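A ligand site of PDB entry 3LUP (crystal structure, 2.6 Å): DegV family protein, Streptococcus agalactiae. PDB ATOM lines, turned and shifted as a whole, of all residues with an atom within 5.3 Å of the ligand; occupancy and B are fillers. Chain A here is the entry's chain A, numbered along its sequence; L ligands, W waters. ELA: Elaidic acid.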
ATOM      1  N   ILE A  31      25.764 -20.091  10.731  1.00  0.00           N
ATOM      2  CA  ILE A  31      26.083 -19.150  11.815  1.00  0.00           C
ATOM      3  C   ILE A  31      27.176 -18.163  11.381  1.00  0.00           C
ATOM      4  O   ILE A  31      28.284 -18.572  11.092  1.00  0.00           O
ATOM      5  CB  ILE A  31      26.514 -19.870  13.125  1.00  0.00           C
ATOM      6  CG1 ILE A  31      25.409 -20.844  13.577  1.00  0.00           C
ATOM      7  CG2 ILE A  31      26.876 -18.846  14.212  1.00  0.00           C
ATOM      8  CD1 ILE A  31      25.729 -21.685  14.789  1.00  0.00           C
ATOM      9  N   THR A  64      30.051 -13.893  17.197  1.00  0.00           N
ATOM     10  CA  THR A  64      29.147 -14.602  16.316  1.00  0.00           C
ATOM     11  C   THR A  64      27.753 -14.020  16.488  1.00  0.00           C
ATOM     12  O   THR A  64      27.499 -13.217  17.404  1.00  0.00           O
ATOM     13  CB  THR A  64      29.117 -16.118  16.602  1.00  0.00           C
ATOM     14  OG1 THR A  64      28.756 -16.334  17.963  1.00  0.00           O
ATOM     15  CG2 THR A  64      30.494 -16.745  16.339  1.00  0.00           C
ATOM     16  N   SER A  65      26.854 -14.379  15.578  1.00  0.00           N
ATOM     17  CA  SER A  65      25.463 -14.009  15.687  1.00  0.00           C
ATOM     18  C   SER A  65      24.628 -15.241  15.458  1.00  0.00           C
ATOM     19  O   SER A  65      25.090 -16.191  14.844  1.00  0.00           O
ATOM     20  CB  SER A  65      25.105 -12.924  14.679  1.00  0.00           C
ATOM     21  OG  SER A  65      25.260 -13.457  13.376  1.00  0.00           O
ATOM     22  N   GLN A  66      23.390 -15.208  15.967  1.00  0.00           N
ATOM     23  CA  GLN A  66      22.431 -16.293  15.809  1.00  0.00           C
ATOM     24  C   GLN A  66      22.189 -16.534  14.322  1.00  0.00           C
ATOM     25  O   GLN A  66      22.315 -15.611  13.524  1.00  0.00           O
ATOM     26  CB  GLN A  66      21.111 -15.913  16.483  1.00  0.00           C
ATOM     27  CG  GLN A  66      21.187 -15.846  17.993  1.00  0.00           C
ATOM     28  CD  GLN A  66      20.005 -15.143  18.624  1.00  0.00           C
ATOM     29  OE1 GLN A  66      18.837 -15.402  18.288  1.00  0.00           O
ATOM     30  NE2 GLN A  66      20.295 -14.246  19.564  1.00  0.00           N
ATOM     31  N   PRO A  67      21.880 -17.791  13.942  1.00  0.00           N
ATOM     32  CA  PRO A  67      21.422 -17.984  12.559  1.00  0.00           C
ATOM     33  C   PRO A  67      20.178 -17.152  12.286  1.00  0.00           C
ATOM     34  O   PRO A  67      19.526 -16.696  13.222  1.00  0.00           O
ATOM     35  CB  PRO A  67      21.118 -19.487  12.479  1.00  0.00           C
ATOM     36  CG  PRO A  67      21.389 -20.046  13.821  1.00  0.00           C
ATOM     37  CD  PRO A  67      22.167 -19.062  14.615  1.00  0.00           C
ATOM     38  N   ILE A  92      22.199 -25.413  18.487  1.00  0.00           N
ATOM     39  CA  ILE A  92      23.061 -24.939  19.562  1.00  0.00           C
ATOM     40  C   ILE A  92      22.325 -24.675  20.911  1.00  0.00           C
ATOM     41  O   ILE A  92      21.197 -24.165  20.947  1.00  0.00           O
ATOM     42  CB  ILE A  92      23.827 -23.684  19.047  1.00  0.00           C
ATOM     43  CG1 ILE A  92      24.901 -23.217  20.026  1.00  0.00           C
ATOM     44  CG2 ILE A  92      22.881 -22.535  18.718  1.00  0.00           C
ATOM     45  CD1 ILE A  92      26.096 -22.558  19.347  1.00  0.00           C
ATOM     46  N   ILE A  96      24.064 -20.881  25.570  1.00  0.00           N
ATOM     47  CA  ILE A  96      25.210 -20.229  24.927  1.00  0.00           C
ATOM     48  C   ILE A  96      24.805 -19.391  23.714  1.00  0.00           C
ATOM     49  O   ILE A  96      25.657 -18.998  22.915  1.00  0.00           O
ATOM     50  CB  ILE A  96      26.316 -21.254  24.519  1.00  0.00           C
ATOM     51  CG1 ILE A  96      25.820 -22.194  23.423  1.00  0.00           C
ATOM     52  CG2 ILE A  96      26.817 -22.046  25.744  1.00  0.00           C
ATOM     53  CD1 ILE A  96      26.891 -23.079  22.879  1.00  0.00           C
ATOM     54  N   SER A  97      23.511 -19.124  23.602  1.00  0.00           N
ATOM     55  CA  SER A  97      22.928 -18.413  22.461  1.00  0.00           C
ATOM     56  C   SER A  97      21.437 -18.363  22.687  1.00  0.00           C
ATOM     57  O   SER A  97      20.832 -19.381  23.059  1.00  0.00           O
ATOM     58  CB  SER A  97      23.198 -19.164  21.156  1.00  0.00           C
ATOM     59  OG  SER A  97      22.940 -18.344  20.053  1.00  0.00           O
ATOM     60  N   GLY A  98      20.839 -17.196  22.457  1.00  0.00           N
ATOM     61  CA  GLY A  98      19.401 -17.022  22.624  1.00  0.00           C
ATOM     62  C   GLY A  98      18.609 -17.434  21.414  1.00  0.00           C
ATOM     63  O   GLY A  98      17.437 -17.084  21.278  1.00  0.00           O
ATOM     64  N   ILE A 122      23.816 -28.551  24.130  1.00  0.00           N
ATOM     65  CA  ILE A 122      25.163 -28.893  23.688  1.00  0.00           C
ATOM     66  C   ILE A 122      25.465 -28.287  22.309  1.00  0.00           C
ATOM     67  O   ILE A 122      24.711 -27.429  21.826  1.00  0.00           O
ATOM     68  CB  ILE A 122      25.422 -30.429  23.777  1.00  0.00           C
ATOM     69  CG1 ILE A 122      26.911 -30.729  23.894  1.00  0.00           C
ATOM     70  CG2 ILE A 122      24.654 -31.225  22.695  1.00  0.00           C
ATOM     71  CD1 ILE A 122      27.491 -30.299  25.271  1.00  0.00           C
ATOM     72  N   THR A 123      26.571 -28.693  21.714  1.00  0.00           N
ATOM     73  CA  THR A 123      26.919 -28.240  20.381  1.00  0.00           C
ATOM     74  C   THR A 123      28.005 -29.164  19.845  1.00  0.00           C
ATOM     75  O   THR A 123      28.251 -30.209  20.419  1.00  0.00           O
ATOM     76  CB  THR A 123      27.331 -26.727  20.372  1.00  0.00           C
ATOM     77  OG1 THR A 123      27.428 -26.265  19.026  1.00  0.00           O
ATOM     78  CG2 THR A 123      28.654 -26.492  21.097  1.00  0.00           C
ATOM     79  N   SER A 124      28.634 -28.797  18.739  1.00  0.00           N
ATOM     80  CA  SER A 124      29.699 -29.617  18.161  1.00  0.00           C
ATOM     81  C   SER A 124      29.179 -31.049  17.935  1.00  0.00           C
ATOM     82  O   SER A 124      28.058 -31.222  17.427  1.00  0.00           O
ATOM     83  CB  SER A 124      30.948 -29.583  19.048  1.00  0.00           C
ATOM     84  OG  SER A 124      31.991 -30.367  18.505  1.00  0.00           O
ATOM     85  N   PRO A 126      28.301 -33.949  19.874  1.00  0.00           N
ATOM     86  CA  PRO A 126      27.073 -34.482  20.455  1.00  0.00           C
ATOM     87  C   PRO A 126      25.811 -33.996  19.728  1.00  0.00           C
ATOM     88  O   PRO A 126      24.875 -34.780  19.536  1.00  0.00           O
ATOM     89  CB  PRO A 126      27.117 -33.942  21.889  1.00  0.00           C
ATOM     90  CG  PRO A 126      28.551 -33.988  22.219  1.00  0.00           C
ATOM     91  CD  PRO A 126      29.217 -33.495  20.941  1.00  0.00           C
ATOM     92  N   GLU A 159      27.370 -35.107  27.588  1.00  0.00           N
ATOM     93  CA  GLU A 159      28.251 -34.351  28.451  1.00  0.00           C
ATOM     94  C   GLU A 159      29.261 -33.673  27.552  1.00  0.00           C
ATOM     95  O   GLU A 159      29.635 -34.216  26.518  1.00  0.00           O
ATOM     96  CB  GLU A 159      29.014 -35.288  29.398  1.00  0.00           C
ATOM     97  CG  GLU A 159      28.132 -36.113  30.357  1.00  0.00           C
ATOM     98  CD  GLU A 159      27.408 -35.273  31.433  1.00  0.00           C
ATOM     99  OE1 GLU A 159      27.921 -34.194  31.864  1.00  0.00           O
ATOM    100  OE2 GLU A 159      26.315 -35.723  31.867  1.00  0.00           O
ATOM    101  N   GLY A 160      29.721 -32.487  27.964  1.00  0.00           N
ATOM    102  CA  GLY A 160      30.729 -31.756  27.217  1.00  0.00           C
ATOM    103  C   GLY A 160      31.679 -31.075  28.169  1.00  0.00           C
ATOM    104  O   GLY A 160      31.279 -30.175  28.897  1.00  0.00           O
ATOM    105  N   PHE A 161      32.932 -31.523  28.169  1.00  0.00           N
ATOM    106  CA  PHE A 161      33.969 -30.972  29.047  1.00  0.00           C
ATOM    107  C   PHE A 161      35.075 -30.320  28.222  1.00  0.00           C
ATOM    108  O   PHE A 161      35.415 -30.789  27.149  1.00  0.00           O
ATOM    109  CB  PHE A 161      34.523 -32.088  29.937  1.00  0.00           C
ATOM    110  CG  PHE A 161      33.595 -32.462  31.068  1.00  0.00           C
ATOM    111  CD1 PHE A 161      33.917 -32.121  32.395  1.00  0.00           C
ATOM    112  CD2 PHE A 161      32.416 -33.152  30.831  1.00  0.00           C
ATOM    113  CE1 PHE A 161      33.064 -32.453  33.454  1.00  0.00           C
ATOM    114  CE2 PHE A 161      31.556 -33.494  31.897  1.00  0.00           C
ATOM    115  CZ  PHE A 161      31.885 -33.143  33.217  1.00  0.00           C
ATOM    116  N   ILE A 162      35.637 -29.225  28.739  1.00  0.00           N
ATOM    117  CA  ILE A 162      36.554 -28.378  27.973  1.00  0.00           C
ATOM    118  C   ILE A 162      37.715 -27.897  28.827  1.00  0.00           C
ATOM    119  O   ILE A 162      37.549 -27.589  29.993  1.00  0.00           O
ATOM    120  CB  ILE A 162      35.861 -27.082  27.429  1.00  0.00           C
ATOM    121  CG1 ILE A 162      34.398 -27.328  27.049  1.00  0.00           C
ATOM    122  CG2 ILE A 162      36.672 -26.474  26.263  1.00  0.00           C
ATOM    123  CD1 ILE A 162      33.513 -26.088  27.227  1.00  0.00           C
ATOM    124  N   LEU A 170      36.241 -17.042  26.314  1.00  0.00           N
ATOM    125  CA  LEU A 170      35.087 -17.472  27.083  1.00  0.00           C
ATOM    126  C   LEU A 170      34.477 -16.419  28.003  1.00  0.00           C
ATOM    127  O   LEU A 170      33.255 -16.345  28.124  1.00  0.00           O
ATOM    128  CB  LEU A 170      35.389 -18.735  27.868  1.00  0.00           C
ATOM    129  CG  LEU A 170      35.030 -20.029  27.134  1.00  0.00           C
ATOM    130  CD1 LEU A 170      35.359 -21.230  27.987  1.00  0.00           C
ATOM    131  CD2 LEU A 170      33.559 -20.058  26.721  1.00  0.00           C
ATOM    132  N   ARG A 175      30.291 -16.537  27.225  1.00  0.00           N
ATOM    133  CA  ARG A 175      29.645 -17.861  27.337  1.00  0.00           C
ATOM    134  C   ARG A 175      30.038 -18.632  28.596  1.00  0.00           C
ATOM    135  O   ARG A 175      29.342 -19.582  28.969  1.00  0.00           O
ATOM    136  CB  ARG A 175      29.820 -18.720  26.080  1.00  0.00           C
ATOM    137  CG  ARG A 175      29.650 -17.991  24.760  1.00  0.00           C
ATOM    138  CD  ARG A 175      28.231 -17.567  24.449  1.00  0.00           C
ATOM    139  NE  ARG A 175      28.288 -16.369  23.611  1.00  0.00           N
ATOM    140  CZ  ARG A 175      27.306 -15.897  22.852  1.00  0.00           C
ATOM    141  NH1 ARG A 175      26.144 -16.510  22.774  1.00  0.00           N
ATOM    142  NH2 ARG A 175      27.497 -14.794  22.149  1.00  0.00           N
ATOM    143  N   PHE A 195      29.321 -28.328  30.497  1.00  0.00           N
ATOM    144  CA  PHE A 195      27.957 -27.838  30.332  1.00  0.00           C
ATOM    145  C   PHE A 195      27.049 -28.195  31.508  1.00  0.00           C
ATOM    146  O   PHE A 195      26.961 -29.362  31.905  1.00  0.00           O
ATOM    147  CB  PHE A 195      27.351 -28.356  29.050  1.00  0.00           C
ATOM    148  CG  PHE A 195      27.750 -27.569  27.830  1.00  0.00           C
ATOM    149  CD1 PHE A 195      26.811 -26.753  27.188  1.00  0.00           C
ATOM    150  CD2 PHE A 195      29.037 -27.663  27.310  1.00  0.00           C
ATOM    151  CE1 PHE A 195      27.154 -26.026  26.053  1.00  0.00           C
ATOM    152  CE2 PHE A 195      29.403 -26.926  26.171  1.00  0.00           C
ATOM    153  CZ  PHE A 195      28.447 -26.108  25.540  1.00  0.00           C
ATOM    154  N   ILE A 201      27.957 -23.007  30.200  1.00  0.00           N
ATOM    155  CA  ILE A 201      29.311 -23.385  30.499  1.00  0.00           C
ATOM    156  C   ILE A 201      29.700 -22.815  31.848  1.00  0.00           C
ATOM    157  O   ILE A 201      29.616 -21.599  32.065  1.00  0.00           O
ATOM    158  CB  ILE A 201      30.297 -22.978  29.432  1.00  0.00           C
ATOM    159  CG1 ILE A 201      29.753 -23.359  28.033  1.00  0.00           C
ATOM    160  CG2 ILE A 201      31.657 -23.626  29.751  1.00  0.00           C
ATOM    161  CD1 ILE A 201      30.728 -23.078  26.874  1.00  0.00           C
ATOM    162  N   ILE A 235      37.649 -33.093  20.752  1.00  0.00           N
ATOM    163  CA  ILE A 235      37.469 -31.979  19.824  1.00  0.00           C
ATOM    164  C   ILE A 235      38.458 -30.890  20.205  1.00  0.00           C
ATOM    165  O   ILE A 235      38.647 -30.628  21.381  1.00  0.00           O
ATOM    166  CB  ILE A 235      36.027 -31.438  19.876  1.00  0.00           C
ATOM    167  CG1 ILE A 235      35.020 -32.596  19.974  1.00  0.00           C
ATOM    168  CG2 ILE A 235      35.733 -30.556  18.663  1.00  0.00           C
ATOM    169  CD1 ILE A 235      33.934 -32.384  21.009  1.00  0.00           C
ATOM    170  N   PHE A 264      37.022 -28.144  15.900  1.00  0.00           N
ATOM    171  CA  PHE A 264      36.050 -27.064  15.983  1.00  0.00           C
ATOM    172  C   PHE A 264      36.146 -26.217  14.703  1.00  0.00           C
ATOM    173  O   PHE A 264      37.162 -26.269  13.995  1.00  0.00           O
ATOM    174  CB  PHE A 264      36.311 -26.164  17.200  1.00  0.00           C
ATOM    175  CG  PHE A 264      36.078 -26.844  18.545  1.00  0.00           C
ATOM    176  CD1 PHE A 264      34.791 -27.233  18.955  1.00  0.00           C
ATOM    177  CD2 PHE A 264      37.141 -27.049  19.432  1.00  0.00           C
ATOM    178  CE1 PHE A 264      34.576 -27.845  20.213  1.00  0.00           C
ATOM    179  CE2 PHE A 264      36.937 -27.663  20.671  1.00  0.00           C
ATOM    180  CZ  PHE A 264      35.653 -28.055  21.068  1.00  0.00           C
ATOM    181  N   VAL A 267      33.185 -20.739  14.501  1.00  0.00           N
ATOM    182  CA  VAL A 267      32.098 -20.394  15.414  1.00  0.00           C
ATOM    183  C   VAL A 267      32.514 -20.647  16.869  1.00  0.00           C
ATOM    184  O   VAL A 267      32.479 -19.721  17.685  1.00  0.00           O
ATOM    185  CB  VAL A 267      30.790 -21.122  15.027  1.00  0.00           C
ATOM    186  CG1 VAL A 267      29.710 -20.871  16.050  1.00  0.00           C
ATOM    187  CG2 VAL A 267      30.319 -20.660  13.632  1.00  0.00           C
ATOM    188  N   ILE A 268      32.951 -21.870  17.171  1.00  0.00           N
ATOM    189  CA  ILE A 268      33.366 -22.269  18.532  1.00  0.00           C
ATOM    190  C   ILE A 268      34.785 -21.816  18.880  1.00  0.00           C
ATOM    191  O   ILE A 268      35.039 -21.447  20.015  1.00  0.00           O
ATOM    192  CB  ILE A 268      33.157 -23.779  18.769  1.00  0.00           C
ATOM    193  CG1 ILE A 268      31.673 -24.138  18.584  1.00  0.00           C
ATOM    194  CG2 ILE A 268      33.611 -24.184  20.152  1.00  0.00           C
ATOM    195  CD1 ILE A 268      31.374 -25.609  18.383  1.00  0.00           C
ATOM    196  N   HIS A 271      34.717 -18.497  20.561  1.00  0.00           N
ATOM    197  CA  HIS A 271      34.355 -18.420  21.979  1.00  0.00           C
ATOM    198  C   HIS A 271      35.319 -19.161  22.898  1.00  0.00           C
ATOM    199  O   HIS A 271      35.437 -18.859  24.091  1.00  0.00           O
ATOM    200  CB  HIS A 271      32.910 -18.879  22.180  1.00  0.00           C
ATOM    201  CG  HIS A 271      31.923 -17.990  21.496  1.00  0.00           C
ATOM    202  ND1 HIS A 271      31.396 -16.864  22.086  1.00  0.00           N
ATOM    203  CD2 HIS A 271      31.417 -18.024  20.241  1.00  0.00           C
ATOM    204  CE1 HIS A 271      30.581 -16.258  21.237  1.00  0.00           C
ATOM    205  NE2 HIS A 271      30.577 -16.951  20.110  1.00  0.00           N
ATOM    206  N   LEU A 272      36.032 -20.134  22.335  1.00  0.00           N
ATOM    207  CA  LEU A 272      36.939 -20.941  23.108  1.00  0.00           C
ATOM    208  C   LEU A 272      38.377 -20.435  23.015  1.00  0.00           C
ATOM    209  O   LEU A 272      39.171 -20.604  23.948  1.00  0.00           O
ATOM    210  CB  LEU A 272      36.838 -22.395  22.644  1.00  0.00           C
ATOM    211  CG  LEU A 272      36.132 -23.416  23.543  1.00  0.00           C
ATOM    212  CD1 LEU A 272      34.761 -22.956  24.028  1.00  0.00           C
ATOM    213  CD2 LEU A 272      36.062 -24.766  22.829  1.00  0.00           C
ATOM    214  N   ALA A 278      38.567 -30.386  24.174  1.00  0.00           N
ATOM    215  CA  ALA A 278      37.302 -30.739  24.808  1.00  0.00           C
ATOM    216  C   ALA A 278      36.979 -32.192  24.535  1.00  0.00           C
ATOM    217  O   ALA A 278      37.588 -32.803  23.658  1.00  0.00           O
ATOM    218  CB  ALA A 278      36.175 -29.883  24.277  1.00  0.00           C
ATOM    219  N   PHE A 279      36.046 -32.748  25.284  1.00  0.00           N
ATOM    220  CA  PHE A 279      35.403 -33.960  24.819  1.00  0.00           C
ATOM    221  C   PHE A 279      33.886 -33.797  24.870  1.00  0.00           C
ATOM    222  O   PHE A 279      33.366 -32.942  25.604  1.00  0.00           O
ATOM    223  CB  PHE A 279      35.883 -35.220  25.579  1.00  0.00           C
ATOM    224  CG  PHE A 279      35.375 -35.322  26.996  1.00  0.00           C
ATOM    225  CD1 PHE A 279      36.203 -34.980  28.070  1.00  0.00           C
ATOM    226  CD2 PHE A 279      34.096 -35.774  27.264  1.00  0.00           C
ATOM    227  CE1 PHE A 279      35.748 -35.075  29.387  1.00  0.00           C
ATOM    228  CE2 PHE A 279      33.631 -35.871  28.565  1.00  0.00           C
ATOM    229  CZ  PHE A 279      34.459 -35.530  29.639  1.00  0.00           C
ATOM    230  N   GLY A 280      33.196 -34.605  24.081  1.00  0.00           N
ATOM    231  CA  GLY A 280      31.746 -34.706  24.170  1.00  0.00           C
ATOM    232  C   GLY A 280      31.368 -36.168  24.047  1.00  0.00           C
ATOM    233  O   GLY A 280      31.960 -36.892  23.228  1.00  0.00           O
HETATM  234  CA  ELA L   1      24.906 -15.729  19.650  1.00  0.00           C
HETATM  235  C   ELA L   1      24.925 -14.212  19.827  1.00  0.00           C
HETATM  236  O   ELA L   1      25.979 -13.546  20.008  1.00  0.00           O
HETATM  237  C3  ELA L   1      25.657 -16.218  18.418  1.00  0.00           C
HETATM  238  C4  ELA L   1      25.359 -17.682  18.129  1.00  0.00           C
HETATM  239  C5  ELA L   1      26.630 -18.555  18.072  1.00  0.00           C
HETATM  240  C6  ELA L   1      27.050 -19.019  19.465  1.00  0.00           C
HETATM  241  C7  ELA L   1      28.463 -19.570  19.620  1.00  0.00           C
HETATM  242  C8  ELA L   1      28.725 -19.927  21.090  1.00  0.00           C
HETATM  243  C9  ELA L   1      29.604 -21.159  21.223  1.00  0.00           C
HETATM  244  C10 ELA L   1      30.225 -21.552  22.513  1.00  0.00           C
HETATM  245  C11 ELA L   1      31.477 -22.406  22.515  1.00  0.00           C
HETATM  246  C12 ELA L   1      31.385 -23.598  23.461  1.00  0.00           C
HETATM  247  C13 ELA L   1      31.322 -24.929  22.738  1.00  0.00           C
HETATM  248  C14 ELA L   1      31.953 -26.067  23.530  1.00  0.00           C
HETATM  249  C15 ELA L   1      31.929 -27.363  22.701  1.00  0.00           C
HETATM  250  C16 ELA L   1      32.248 -28.622  23.510  1.00  0.00           C
HETATM  251  C17 ELA L   1      31.058 -29.578  23.514  1.00  0.00           C
HETATM  252  C18 ELA L   1      31.491 -31.041  23.443  1.00  0.00           C
HETATM  253  OXT ELA L   1      23.828 -13.588  19.809  1.00  0.00           O
HETATM  254  O   HOH W   1      28.941 -13.103  20.309  1.00  0.00           O
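NH2 of Arg 175 lies within salt-bridge range of O of the ligand, 2.9 Å away. The backbone carbonyl oxygen (O) of Thr 64 sits close to an oxygen (O) of the ligand (3.0 Å).
The guanidinium group of Arg 175 lies close to a ring nitrogen (ND1) of His 271 (3.5 Å). NH1 of Arg 175 sits at hydrogen-bond distance from O of Ile 96 (2.5 Å). The backbone NH (N) of Arg 175 is in hydrogen-bond range of the backbone carbonyl oxygen (O) of Leu 170 (3.1 Å). The side-chain hydroxyl (OG1) of Thr 64 is in hydrogen-bond range of a ring nitrogen (NE2) of His 271, 2.9 Å away. O of His 271 sits at hydrogen-bond distance from N of Leu 170, at 3.0 Å. The backbone carbonyl oxygen of Phe 161 lies within hydrogen-bond range of the backbone NH of Phe 279. The backbone carbonyl oxygen (O) of Ile 235 sits at hydrogen-bond distance from the backbone NH (N) of Ala 278, at 2.8 Å. The backbone carbonyl oxygen (O) of Gly 160 sits at hydrogen-bond distance from the backbone NH (N) of Phe 195 (3.1 Å).
Ile 31 touches the ligand (CG2 to C5, 3.9 Å). C of Ser 65 touches C3 of the ligand, at 3.3 Å. Gln 66 touches the ligand. CD1 of Ile 92 touches C6 of the ligand, 3.7 Å away. CD1 of Ile 96 touches C10 of the ligand, 3.7 Å away. Ser 97 touches the ligand (OG to C4, 3.2 Å). Thr 123 touches the ligand (CG2 to C13, 3.5 Å). Gly 160 touches the ligand. CE2 of Phe 195 touches C14 of the ligand, at 3.8 Å. Ile 201 touches the ligand. Ile 235 touches the ligand. CE1 of Phe 264 touches C15 of the ligand (3.7 Å). Val 267 touches the ligand (CG1 to C7, 3.999 Å). CG2 of Ile 268 touches C13 of the ligand, 3.5 Å away. CD2 of His 271 touches C7 of the ligand, 3.4 Å away. Leu 272 touches the ligand (CD1 to C12, 3.5 Å). Phe 279 touches the ligand. CA of Gly 280 touches C18 of the ligand, 3.7 Å away. Hydrophobic or aromatic side chains that line the ligand: Ile 31, Ile 92, Ile 96, Phe 195, Ile 201, Ile 235, Phe 264, Val 267, Ile 268, His 271 and Leu 272. Of the 30 residues printed, 20 come within 4 Å of the ligand. The nearest printed residue that does not touch the ligand is Ile 162 (4.01 Å).
Water W1 lies within hydrogen-bond range of NH2 of Arg 175, O of the ligand and O of Thr 64.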
